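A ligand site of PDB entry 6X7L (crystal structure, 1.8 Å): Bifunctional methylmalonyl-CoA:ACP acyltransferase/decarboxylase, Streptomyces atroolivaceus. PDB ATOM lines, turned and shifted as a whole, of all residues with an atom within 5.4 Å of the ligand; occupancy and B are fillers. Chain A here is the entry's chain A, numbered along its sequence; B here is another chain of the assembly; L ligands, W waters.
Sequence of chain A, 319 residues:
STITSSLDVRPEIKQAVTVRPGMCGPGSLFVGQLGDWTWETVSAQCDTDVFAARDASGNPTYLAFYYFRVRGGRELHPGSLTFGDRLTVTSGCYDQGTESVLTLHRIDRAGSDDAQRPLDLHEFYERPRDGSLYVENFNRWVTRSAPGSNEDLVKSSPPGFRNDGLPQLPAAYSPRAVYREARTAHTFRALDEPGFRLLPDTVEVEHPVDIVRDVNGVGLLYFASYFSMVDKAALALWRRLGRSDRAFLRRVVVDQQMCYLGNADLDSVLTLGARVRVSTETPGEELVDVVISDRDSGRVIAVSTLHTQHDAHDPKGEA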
ATOM      1  N   TRP A  39     -16.579  28.839   6.556  1.00  0.00           N
ATOM      2  CA  TRP A  39     -16.312  27.665   7.435  1.00  0.00           C
ATOM      3  C   TRP A  39     -15.244  28.065   8.473  1.00  0.00           C
ATOM      4  O   TRP A  39     -15.381  27.639   9.611  1.00  0.00           O
ATOM      5  CB  TRP A  39     -15.928  26.447   6.635  1.00  0.00           C
ATOM      6  CG  TRP A  39     -17.115  25.724   6.076  1.00  0.00           C
ATOM      7  CD1 TRP A  39     -18.334  26.229   5.751  1.00  0.00           C
ATOM      8  CD2 TRP A  39     -17.179  24.339   5.755  1.00  0.00           C
ATOM      9  NE1 TRP A  39     -19.146  25.238   5.300  1.00  0.00           N
ATOM     10  CE2 TRP A  39     -18.462  24.065   5.254  1.00  0.00           C
ATOM     11  CE3 TRP A  39     -16.283  23.275   5.883  1.00  0.00           C
ATOM     12  CZ2 TRP A  39     -18.886  22.788   4.960  1.00  0.00           C
ATOM     13  CZ3 TRP A  39     -16.686  22.023   5.543  1.00  0.00           C
ATOM     14  CH2 TRP A  39     -17.955  21.774   5.089  1.00  0.00           C
ATOM     15  N   LEU A  63     -21.843  21.751   6.922  1.00  0.00           N
ATOM     16  CA  LEU A  63     -22.443  23.070   7.096  1.00  0.00           C
ATOM     17  C   LEU A  63     -22.763  23.581   5.685  1.00  0.00           C
ATOM     18  O   LEU A  63     -21.996  24.387   5.124  1.00  0.00           O
ATOM     19  CB  LEU A  63     -21.519  23.993   7.856  1.00  0.00           C
ATOM     20  CG  LEU A  63     -22.099  25.371   8.168  1.00  0.00           C
ATOM     21  CD1 LEU A  63     -23.493  25.288   8.812  1.00  0.00           C
ATOM     22  CD2 LEU A  63     -21.173  26.210   9.038  1.00  0.00           C
ATOM     23  N   ALA A  64     -23.818  23.051   5.111  1.00  0.00           N
ATOM     24  CA  ALA A  64     -24.170  23.277   3.692  1.00  0.00           C
ATOM     25  C   ALA A  64     -24.562  24.717   3.410  1.00  0.00           C
ATOM     26  O   ALA A  64     -25.310  25.329   4.168  1.00  0.00           O
ATOM     27  CB  ALA A  64     -25.275  22.320   3.310  1.00  0.00           C
ATOM     28  N   PHE A  65     -24.097  25.206   2.265  1.00  0.00           N
ATOM     29  CA  PHE A  65     -24.539  26.514   1.730  1.00  0.00           C
ATOM     30  C   PHE A  65     -26.022  26.405   1.422  1.00  0.00           C
ATOM     31  O   PHE A  65     -26.441  25.445   0.793  1.00  0.00           O
ATOM     32  CB  PHE A  65     -23.626  26.949   0.594  1.00  0.00           C
ATOM     33  CG  PHE A  65     -22.263  27.320   1.132  1.00  0.00           C
ATOM     34  CD1 PHE A  65     -21.275  26.368   1.322  1.00  0.00           C
ATOM     35  CD2 PHE A  65     -22.003  28.636   1.522  1.00  0.00           C
ATOM     36  CE1 PHE A  65     -20.080  26.678   1.950  1.00  0.00           C
ATOM     37  CE2 PHE A  65     -20.810  28.933   2.168  1.00  0.00           C
ATOM     38  CZ  PHE A  65     -19.863  27.975   2.388  1.00  0.00           C
ATOM     39  N   TYR A  66     -26.781  27.421   1.773  1.00  0.00           N
ATOM     40  CA  TYR A  66     -28.244  27.440   1.476  1.00  0.00           C
ATOM     41  C   TYR A  66     -28.687  28.739   0.813  1.00  0.00           C
ATOM     42  O   TYR A  66     -29.393  28.682  -0.202  1.00  0.00           O
ATOM     43  CB  TYR A  66     -29.055  27.136   2.732  1.00  0.00           C
ATOM     44  CG  TYR A  66     -30.486  26.910   2.356  1.00  0.00           C
ATOM     45  CD1 TYR A  66     -30.916  25.701   1.818  1.00  0.00           C
ATOM     46  CD2 TYR A  66     -31.384  27.944   2.410  1.00  0.00           C
ATOM     47  CE1 TYR A  66     -32.229  25.517   1.406  1.00  0.00           C
ATOM     48  CE2 TYR A  66     -32.699  27.766   1.975  1.00  0.00           C
ATOM     49  CZ  TYR A  66     -33.109  26.564   1.432  1.00  0.00           C
ATOM     50  OH  TYR A  66     -34.391  26.415   0.993  1.00  0.00           O
ATOM     51  N   ARG A 140     -26.787  25.724   6.599  1.00  0.00           N
ATOM     52  CA  ARG A 140     -27.612  24.760   7.351  1.00  0.00           C
ATOM     53  C   ARG A 140     -26.831  23.470   7.527  1.00  0.00           C
ATOM     54  O   ARG A 140     -26.413  22.865   6.562  1.00  0.00           O
ATOM     55  CB  ARG A 140     -28.918  24.496   6.601  1.00  0.00           C
ATOM     56  CG  ARG A 140     -29.678  25.765   6.318  1.00  0.00           C
ATOM     57  CD  ARG A 140     -30.915  25.491   5.507  1.00  0.00           C
ATOM     58  NE  ARG A 140     -31.996  25.025   6.359  1.00  0.00           N
ATOM     59  CZ  ARG A 140     -33.278  25.006   5.957  1.00  0.00           C
ATOM     60  NH1 ARG A 140     -33.599  25.440   4.755  1.00  0.00           N
ATOM     61  NH2 ARG A 140     -34.234  24.588   6.743  1.00  0.00           N
ATOM     62  N   VAL A 142     -26.426  19.702   7.660  1.00  0.00           N
ATOM     63  CA  VAL A 142     -27.113  18.520   7.091  1.00  0.00           C
ATOM     64  C   VAL A 142     -26.256  17.268   7.175  1.00  0.00           C
ATOM     65  O   VAL A 142     -25.029  17.356   7.164  1.00  0.00           O
ATOM     66  CB  VAL A 142     -27.537  18.757   5.646  1.00  0.00           C
ATOM     67  CG1 VAL A 142     -28.429  19.988   5.559  1.00  0.00           C
ATOM     68  CG2 VAL A 142     -26.361  18.837   4.709  1.00  0.00           C
ATOM     69  N   LEU A 153     -31.477  15.126   2.138  1.00  0.00           N
ATOM     70  CA  LEU A 153     -30.554  15.443   3.247  1.00  0.00           C
ATOM     71  C   LEU A 153     -31.384  15.809   4.467  1.00  0.00           C
ATOM     72  O   LEU A 153     -32.540  16.271   4.321  1.00  0.00           O
ATOM     73  CB  LEU A 153     -29.605  16.560   2.820  1.00  0.00           C
ATOM     74  CG  LEU A 153     -28.788  16.247   1.555  1.00  0.00           C
ATOM     75  CD1 LEU A 153     -27.898  17.425   1.204  1.00  0.00           C
ATOM     76  CD2 LEU A 153     -27.960  14.978   1.712  1.00  0.00           C
ATOM     77  N   VAL A 154     -30.824  15.533   5.622  1.00  0.00           N
ATOM     78  CA  VAL A 154     -31.495  15.627   6.954  1.00  0.00           C
ATOM     79  C   VAL A 154     -30.865  16.734   7.796  1.00  0.00           C
ATOM     80  O   VAL A 154     -29.619  16.840   7.838  1.00  0.00           O
ATOM     81  CB  VAL A 154     -31.411  14.259   7.650  1.00  0.00           C
ATOM     82  CG1 VAL A 154     -32.184  14.279   8.964  1.00  0.00           C
ATOM     83  CG2 VAL A 154     -31.868  13.164   6.729  1.00  0.00           C
ATOM     84  N   LYS A 155     -31.695  17.543   8.461  1.00  0.00           N
ATOM     85  CA  LYS A 155     -31.194  18.642   9.318  1.00  0.00           C
ATOM     86  C   LYS A 155     -30.453  18.025  10.522  1.00  0.00           C
ATOM     87  O   LYS A 155     -30.764  16.882  10.989  1.00  0.00           O
ATOM     88  CB  LYS A 155     -32.318  19.629   9.670  1.00  0.00           C
ATOM     89  CG  LYS A 155     -33.306  19.141  10.690  1.00  0.00           C
ATOM     90  CD  LYS A 155     -34.269  20.245  11.146  1.00  0.00           C
ATOM     91  CE  LYS A 155     -35.101  20.786  10.006  1.00  0.00           C
ATOM     92  NZ  LYS A 155     -34.439  21.904   9.284  1.00  0.00           N
ATOM     93  N   ARG A 183     -37.814  30.688  -3.783  1.00  0.00           N
ATOM     94  CA  ARG A 183     -38.261  29.307  -4.137  1.00  0.00           C
ATOM     95  C   ARG A 183     -39.641  29.345  -4.805  1.00  0.00           C
ATOM     96  O   ARG A 183     -39.955  28.424  -5.617  1.00  0.00           O
ATOM     97  CB  ARG A 183     -38.392  28.442  -2.894  1.00  0.00           C
ATOM     98  CG  ARG A 183     -37.092  28.280  -2.140  1.00  0.00           C
ATOM     99  CD  ARG A 183     -37.231  27.218  -1.070  1.00  0.00           C
ATOM    100  NE  ARG A 183     -38.290  27.512  -0.099  1.00  0.00           N
ATOM    101  CZ  ARG A 183     -38.243  27.229   1.201  1.00  0.00           C
ATOM    102  NH1 ARG A 183     -37.163  26.703   1.774  1.00  0.00           N
ATOM    103  NH2 ARG A 183     -39.282  27.502   1.961  1.00  0.00           N
ATOM    104  N   ASN A 216     -17.448  17.650  -4.935  1.00  0.00           N
ATOM    105  CA  ASN A 216     -16.619  18.087  -3.793  1.00  0.00           C
ATOM    106  C   ASN A 216     -15.976  16.880  -3.101  1.00  0.00           C
ATOM    107  O   ASN A 216     -16.145  15.704  -3.536  1.00  0.00           O
ATOM    108  CB  ASN A 216     -17.399  18.996  -2.831  1.00  0.00           C
ATOM    109  CG  ASN A 216     -18.407  18.286  -1.943  1.00  0.00           C
ATOM    110  OD1 ASN A 216     -18.394  17.052  -1.858  1.00  0.00           O
ATOM    111  ND2 ASN A 216     -19.310  19.061  -1.348  1.00  0.00           N
ATOM    112  N   LEU A 220     -20.678  15.298  -2.741  1.00  0.00           N
ATOM    113  CA  LEU A 220     -21.841  16.163  -3.101  1.00  0.00           C
ATOM    114  C   LEU A 220     -21.476  16.999  -4.333  1.00  0.00           C
ATOM    115  O   LEU A 220     -20.287  17.168  -4.605  1.00  0.00           O
ATOM    116  CB  LEU A 220     -22.141  17.095  -1.952  1.00  0.00           C
ATOM    117  CG  LEU A 220     -22.624  16.403  -0.668  1.00  0.00           C
ATOM    118  CD1 LEU A 220     -22.658  17.409   0.442  1.00  0.00           C
ATOM    119  CD2 LEU A 220     -24.003  15.801  -0.855  1.00  0.00           C
ATOM    120  N   LEU A 221     -22.476  17.569  -5.011  1.00  0.00           N
ATOM    121  CA  LEU A 221     -22.214  18.686  -5.942  1.00  0.00           C
ATOM    122  C   LEU A 221     -21.599  19.819  -5.127  1.00  0.00           C
ATOM    123  O   LEU A 221     -22.108  20.154  -4.049  1.00  0.00           O
ATOM    124  CB  LEU A 221     -23.494  19.194  -6.606  1.00  0.00           C
ATOM    125  CG  LEU A 221     -24.246  18.195  -7.487  1.00  0.00           C
ATOM    126  CD1 LEU A 221     -25.476  18.882  -8.047  1.00  0.00           C
ATOM    127  CD2 LEU A 221     -23.327  17.698  -8.583  1.00  0.00           C
ATOM    128  N   TYR A 222     -20.499  20.361  -5.614  1.00  0.00           N
ATOM    129  CA  TYR A 222     -19.741  21.411  -4.911  1.00  0.00           C
ATOM    130  C   TYR A 222     -20.474  22.745  -4.981  1.00  0.00           C
ATOM    131  O   TYR A 222     -20.976  23.135  -6.055  1.00  0.00           O
ATOM    132  CB  TYR A 222     -18.396  21.525  -5.604  1.00  0.00           C
ATOM    133  CG  TYR A 222     -17.459  22.589  -5.073  1.00  0.00           C
ATOM    134  CD1 TYR A 222     -17.139  22.640  -3.724  1.00  0.00           C
ATOM    135  CD2 TYR A 222     -16.710  23.366  -5.937  1.00  0.00           C
ATOM    136  CE1 TYR A 222     -16.241  23.566  -3.218  1.00  0.00           C
ATOM    137  CE2 TYR A 222     -15.773  24.248  -5.464  1.00  0.00           C
ATOM    138  CZ  TYR A 222     -15.560  24.390  -4.104  1.00  0.00           C
ATOM    139  OH  TYR A 222     -14.611  25.298  -3.673  1.00  0.00           O
ATOM    140  N   PHE A 223     -20.564  23.419  -3.837  1.00  0.00           N
ATOM    141  CA  PHE A 223     -21.432  24.604  -3.772  1.00  0.00           C
ATOM    142  C   PHE A 223     -20.978  25.626  -4.809  1.00  0.00           C
ATOM    143  O   PHE A 223     -21.815  26.362  -5.379  1.00  0.00           O
ATOM    144  CB  PHE A 223     -21.394  25.242  -2.372  1.00  0.00           C
ATOM    145  CG  PHE A 223     -20.152  26.022  -2.027  1.00  0.00           C
ATOM    146  CD1 PHE A 223     -18.996  25.403  -1.584  1.00  0.00           C
ATOM    147  CD2 PHE A 223     -20.146  27.418  -2.144  1.00  0.00           C
ATOM    148  CE1 PHE A 223     -17.861  26.148  -1.307  1.00  0.00           C
ATOM    149  CE2 PHE A 223     -18.981  28.137  -1.937  1.00  0.00           C
ATOM    150  CZ  PHE A 223     -17.861  27.515  -1.434  1.00  0.00           C
ATOM    151  N   ALA A 224     -19.689  25.754  -5.083  1.00  0.00           N
ATOM    152  CA  ALA A 224     -19.239  26.833  -6.002  1.00  0.00           C
ATOM    153  C   ALA A 224     -19.633  26.455  -7.436  1.00  0.00           C
ATOM    154  O   ALA A 224     -19.768  27.338  -8.251  1.00  0.00           O
ATOM    155  CB  ALA A 224     -17.750  27.101  -5.855  1.00  0.00           C
ATOM    156  N   TYR A 226     -22.419  25.485  -8.406  1.00  0.00           N
ATOM    157  CA  TYR A 226     -23.755  26.068  -8.698  1.00  0.00           C
ATOM    158  C   TYR A 226     -23.601  27.404  -9.417  1.00  0.00           C
ATOM    159  O   TYR A 226     -24.371  27.684 -10.351  1.00  0.00           O
ATOM    160  CB  TYR A 226     -24.644  26.178  -7.473  1.00  0.00           C
ATOM    161  CG  TYR A 226     -25.175  24.847  -6.984  1.00  0.00           C
ATOM    162  CD1 TYR A 226     -24.344  23.891  -6.416  1.00  0.00           C
ATOM    163  CD2 TYR A 226     -26.541  24.673  -6.849  1.00  0.00           C
ATOM    164  CE1 TYR A 226     -24.872  22.740  -5.886  1.00  0.00           C
ATOM    165  CE2 TYR A 226     -27.095  23.513  -6.344  1.00  0.00           C
ATOM    166  CZ  TYR A 226     -26.247  22.537  -5.849  1.00  0.00           C
ATOM    167  OH  TYR A 226     -26.784  21.423  -5.294  1.00  0.00           O
ATOM    168  N   TYR A 260     -29.749  27.263  -2.633  1.00  0.00           N
ATOM    169  CA  TYR A 260     -29.418  25.845  -2.837  1.00  0.00           C
ATOM    170  C   TYR A 260     -30.566  24.995  -2.282  1.00  0.00           C
ATOM    171  O   TYR A 260     -30.588  24.636  -1.124  1.00  0.00           O
ATOM    172  CB  TYR A 260     -28.120  25.489  -2.123  1.00  0.00           C
ATOM    173  CG  TYR A 260     -26.868  26.176  -2.608  1.00  0.00           C
ATOM    174  CD1 TYR A 260     -26.547  27.436  -2.127  1.00  0.00           C
ATOM    175  CD2 TYR A 260     -25.992  25.558  -3.485  1.00  0.00           C
ATOM    176  CE1 TYR A 260     -25.386  28.070  -2.526  1.00  0.00           C
ATOM    177  CE2 TYR A 260     -24.816  26.152  -3.857  1.00  0.00           C
ATOM    178  CZ  TYR A 260     -24.554  27.448  -3.443  1.00  0.00           C
ATOM    179  OH  TYR A 260     -23.401  28.091  -3.814  1.00  0.00           O
ATOM    180  N   LEU A 261     -31.618  24.797  -3.071  1.00  0.00           N
ATOM    181  CA  LEU A 261     -32.807  24.025  -2.613  1.00  0.00           C
ATOM    182  C   LEU A 261     -32.496  22.545  -2.477  1.00  0.00           C
ATOM    183  O   LEU A 261     -33.130  21.872  -1.677  1.00  0.00           O
ATOM    184  CB  LEU A 261     -33.972  24.204  -3.556  1.00  0.00           C
ATOM    185  CG  LEU A 261     -34.664  25.563  -3.594  1.00  0.00           C
ATOM    186  CD1 LEU A 261     -33.908  26.532  -4.452  1.00  0.00           C
ATOM    187  CD2 LEU A 261     -36.054  25.336  -4.186  1.00  0.00           C
ATOM    188  N   GLY A 262     -31.564  22.027  -3.255  1.00  0.00           N
ATOM    189  CA  GLY A 262     -31.226  20.616  -3.156  1.00  0.00           C
ATOM    190  C   GLY A 262     -29.837  20.358  -3.713  1.00  0.00           C
ATOM    191  O   GLY A 262     -29.266  21.229  -4.406  1.00  0.00           O
ATOM    192  N   ASN A 263     -29.301  19.216  -3.365  1.00  0.00           N
ATOM    193  CA  ASN A 263     -28.091  18.664  -4.010  1.00  0.00           C
ATOM    194  C   ASN A 263     -28.577  17.613  -5.008  1.00  0.00           C
ATOM    195  O   ASN A 263     -29.805  17.551  -5.331  1.00  0.00           O
ATOM    196  CB  ASN A 263     -27.107  18.120  -2.969  1.00  0.00           C
ATOM    197  CG  ASN A 263     -25.673  18.265  -3.438  1.00  0.00           C
ATOM    198  OD1 ASN A 263     -25.195  17.382  -4.139  1.00  0.00           O
ATOM    199  ND2 ASN A 263     -25.010  19.393  -3.118  1.00  0.00           N
ATOM    200  N   PRO B  21     -13.009  22.607   1.871  1.00  0.00           N
ATOM    201  CA  PRO B  21     -13.726  22.299   0.616  1.00  0.00           C
ATOM    202  C   PRO B  21     -13.031  22.806  -0.649  1.00  0.00           C
ATOM    203  O   PRO B  21     -13.092  22.178  -1.697  1.00  0.00           O
ATOM    204  CB  PRO B  21     -15.069  23.013   0.786  1.00  0.00           C
ATOM    205  CG  PRO B  21     -15.256  22.961   2.318  1.00  0.00           C
ATOM    206  CD  PRO B  21     -13.872  23.241   2.877  1.00  0.00           C
ATOM    207  N   PHE B  83     -12.649  16.520   3.828  1.00  0.00           N
ATOM    208  CA  PHE B  83     -12.884  17.680   4.671  1.00  0.00           C
ATOM    209  C   PHE B  83     -12.379  17.380   6.101  1.00  0.00           C
ATOM    210  O   PHE B  83     -12.804  16.364   6.709  1.00  0.00           O
ATOM    211  CB  PHE B  83     -14.376  17.978   4.707  1.00  0.00           C
ATOM    212  CG  PHE B  83     -14.990  18.492   3.426  1.00  0.00           C
ATOM    213  CD1 PHE B  83     -14.277  18.609   2.247  1.00  0.00           C
ATOM    214  CD2 PHE B  83     -16.328  18.855   3.428  1.00  0.00           C
ATOM    215  CE1 PHE B  83     -14.907  19.039   1.086  1.00  0.00           C
ATOM    216  CE2 PHE B  83     -16.940  19.322   2.278  1.00  0.00           C
ATOM    217  CZ  PHE B  83     -16.229  19.374   1.098  1.00  0.00           C
HETATM  218  O1  LIG L   1     -36.056  20.927   6.847  1.00  0.00           O
HETATM  219  P1  LIG L   1     -37.022  20.360   5.709  1.00  0.00           P
HETATM  220  O2  LIG L   1     -36.874  18.878   5.360  1.00  0.00           O
HETATM  221  O3  LIG L   1     -38.505  20.784   5.924  1.00  0.00           O
HETATM  222  O4  LIG L   1     -36.626  21.197   4.387  1.00  0.00           O
HETATM  223  P2  LIG L   1     -36.120  20.551   3.021  1.00  0.00           P
HETATM  224  O5  LIG L   1     -36.388  19.110   2.663  1.00  0.00           O
HETATM  225  O6  LIG L   1     -36.391  21.638   2.013  1.00  0.00           O
HETATM  226  O7  LIG L   1     -34.500  20.459   3.149  1.00  0.00           O
HETATM  227  C1  LIG L   1     -33.707  21.517   3.645  1.00  0.00           C
HETATM  228  C2  LIG L   1     -32.311  21.097   3.106  1.00  0.00           C
HETATM  229  C3  LIG L   1     -31.928  19.700   3.600  1.00  0.00           C
HETATM  230  C4  LIG L   1     -31.289  22.119   3.625  1.00  0.00           C
HETATM  231  C5  LIG L   1     -32.401  21.115   1.568  1.00  0.00           C
HETATM  232  O8  LIG L   1     -32.912  22.367   1.075  1.00  0.00           O
HETATM  233  C6  LIG L   1     -31.092  20.788   0.867  1.00  0.00           C
HETATM  234  O9  LIG L   1     -30.633  19.634   0.764  1.00  0.00           O
HETATM  235  N1  LIG L   1     -30.494  21.821   0.259  1.00  0.00           N
HETATM  236  C7  LIG L   1     -29.275  21.617  -0.484  1.00  0.00           C
HETATM  237  C8  LIG L   1     -28.082  22.304   0.171  1.00  0.00           C
HETATM  238  C9  LIG L   1     -26.860  22.066  -0.651  1.00  0.00           C
HETATM  239  O10 LIG L   1     -26.726  21.036  -1.329  1.00  0.00           O
HETATM  240  N2  LIG L   1     -25.865  22.952  -0.551  1.00  0.00           N
HETATM  241  C10 LIG L   1     -24.553  22.819  -1.108  1.00  0.00           C
HETATM  242  C11 LIG L   1     -23.812  21.562  -0.548  1.00  0.00           C
HETATM  243  S1  LIG L   1     -22.107  21.546  -0.975  1.00  0.00           S
HETATM  244  C12 LIG L   1     -21.431  22.514   0.290  1.00  0.00           C
HETATM  245  O11 LIG L   1     -22.092  23.116   1.082  1.00  0.00           O
HETATM  246  C13 LIG L   1     -19.953  22.509   0.488  1.00  0.00           C
HETATM  247  C14 LIG L   1     -19.312  23.151   1.677  1.00  0.00           C
HETATM  248  N3  LIG L   1     -19.106  22.097  -0.575  1.00  0.00           N
HETATM  249  O12 LIG L   1     -17.857  22.124  -0.358  1.00  0.00           O
HETATM  250  O13 LIG L   1     -19.642  21.719  -1.665  1.00  0.00           O
HETATM  251  O   HOH W   1     -34.692  18.003   0.031  1.00  0.00           O
HETATM  252  O   HOH W   2     -35.408  23.812   0.179  1.00  0.00           O
HETATM  253  O   HOH W   3     -38.297  21.124   0.199  1.00  0.00           O
HETATM  254  O   HOH W   4     -34.577  16.573   2.658  1.00  0.00           O
HETATM  255  O   HOH W   5     -32.012  17.450   0.358  1.00  0.00           O
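The side-chain amide nitrogen (ND2) of Asn 216 is in hydrogen-bond range of an oxygen (O13) of the ligand.
O of Leu 261 is in hydrogen-bond range of O8 of the ligand (2.8 Å).
An oxygen (O11) of the ligand lies within hydrogen-bond range of the backbone NH (N) of Phe 65, at 3.1 Å.
O of Phe 65 is in hydrogen-bond range of N2 of the ligand, 2.9 Å away.
An oxygen (O13) of the ligand is in hydrogen-bond range of the backbone NH of Phe 223, at 2.9 Å.
An oxygen (O10) of the ligand sits at hydrogen-bond distance from the side-chain amide nitrogen (ND2) of Asn 263 (3.0 Å).
The side-chain amino group of Lys 155 is in salt-bridge range of an oxygen (O1) of the ligand.
N1 of the ligand lies within hydrogen-bond range of O of Tyr 260, 3.1 Å away.
The backbone carbonyl oxygen (O) of Leu 221 lies close to a sulfur (S1) of the ligand (3.4 Å).
Trp 39 touches the ligand.
Ala 64 touches the ligand.
Tyr 66 touches the ligand.
Arg 140 touches the ligand.
CD1 of Leu 153 touches O9 of the ligand, 3.5 Å away.
Tyr 222 touches the ligand (CA to O13, 3.3 Å).
Tyr 226 touches the ligand (OH to O10, 3.98 Å).
Gly 262 touches the ligand.
Pro 21 of chain B touches the ligand.
Phe 83 of chain B touches the ligand (CZ to O12, 3.5 Å).
Within 4 Å of the ligand: Trp 39, Ala 64, Phe 65, Tyr 66, Arg 140, Leu 153, Lys 155, Asn 216, Leu 221, Tyr 222, Phe 223, Tyr 226, Tyr 260, Leu 261, Gly 262, Asn 263, Pro 21 of chain B and Phe 83 of chain B.
OD1 of Asn 216 lies within hydrogen-bond range of N of Leu 220 (3.0 Å).
The backbone carbonyl oxygen (O) of Phe 223 lies within hydrogen-bond range of the side-chain hydroxyl (OH) of Tyr 260 (2.8 Å).
OD1 of Asn 263 is in hydrogen-bond range of N of Leu 221 (2.9 Å).
The side-chain amide nitrogen (ND2) of Asn 263 sits close to the side-chain hydroxyl (OH) of Tyr 226, at 3.5 Å.
NH1 of Arg 183 lies within hydrogen-bond range of OH of Tyr 66.
NE1 of Trp 39 sits at hydrogen-bond distance from O of Leu 63 (3.0 Å).
The backbone carbonyl oxygen of Ala 64 is in hydrogen-bond range of the backbone NH of Arg 140.
The side-chain hydroxyl of Tyr 226 is in hydrogen-bond range of the backbone carbonyl oxygen of Gly 262.
Water W5 bridges an oxygen (O9) of the ligand (2.6 Å) and the backbone NH (N) of Leu 153 (3.0 Å).
Water W2 lies within hydrogen-bond range of the side-chain hydroxyl (OH) of Tyr 66 and an oxygen (O6) of the ligand.
Water W4 bridges the backbone carbonyl oxygen of Leu 153 and an oxygen (O5) of the ligand.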
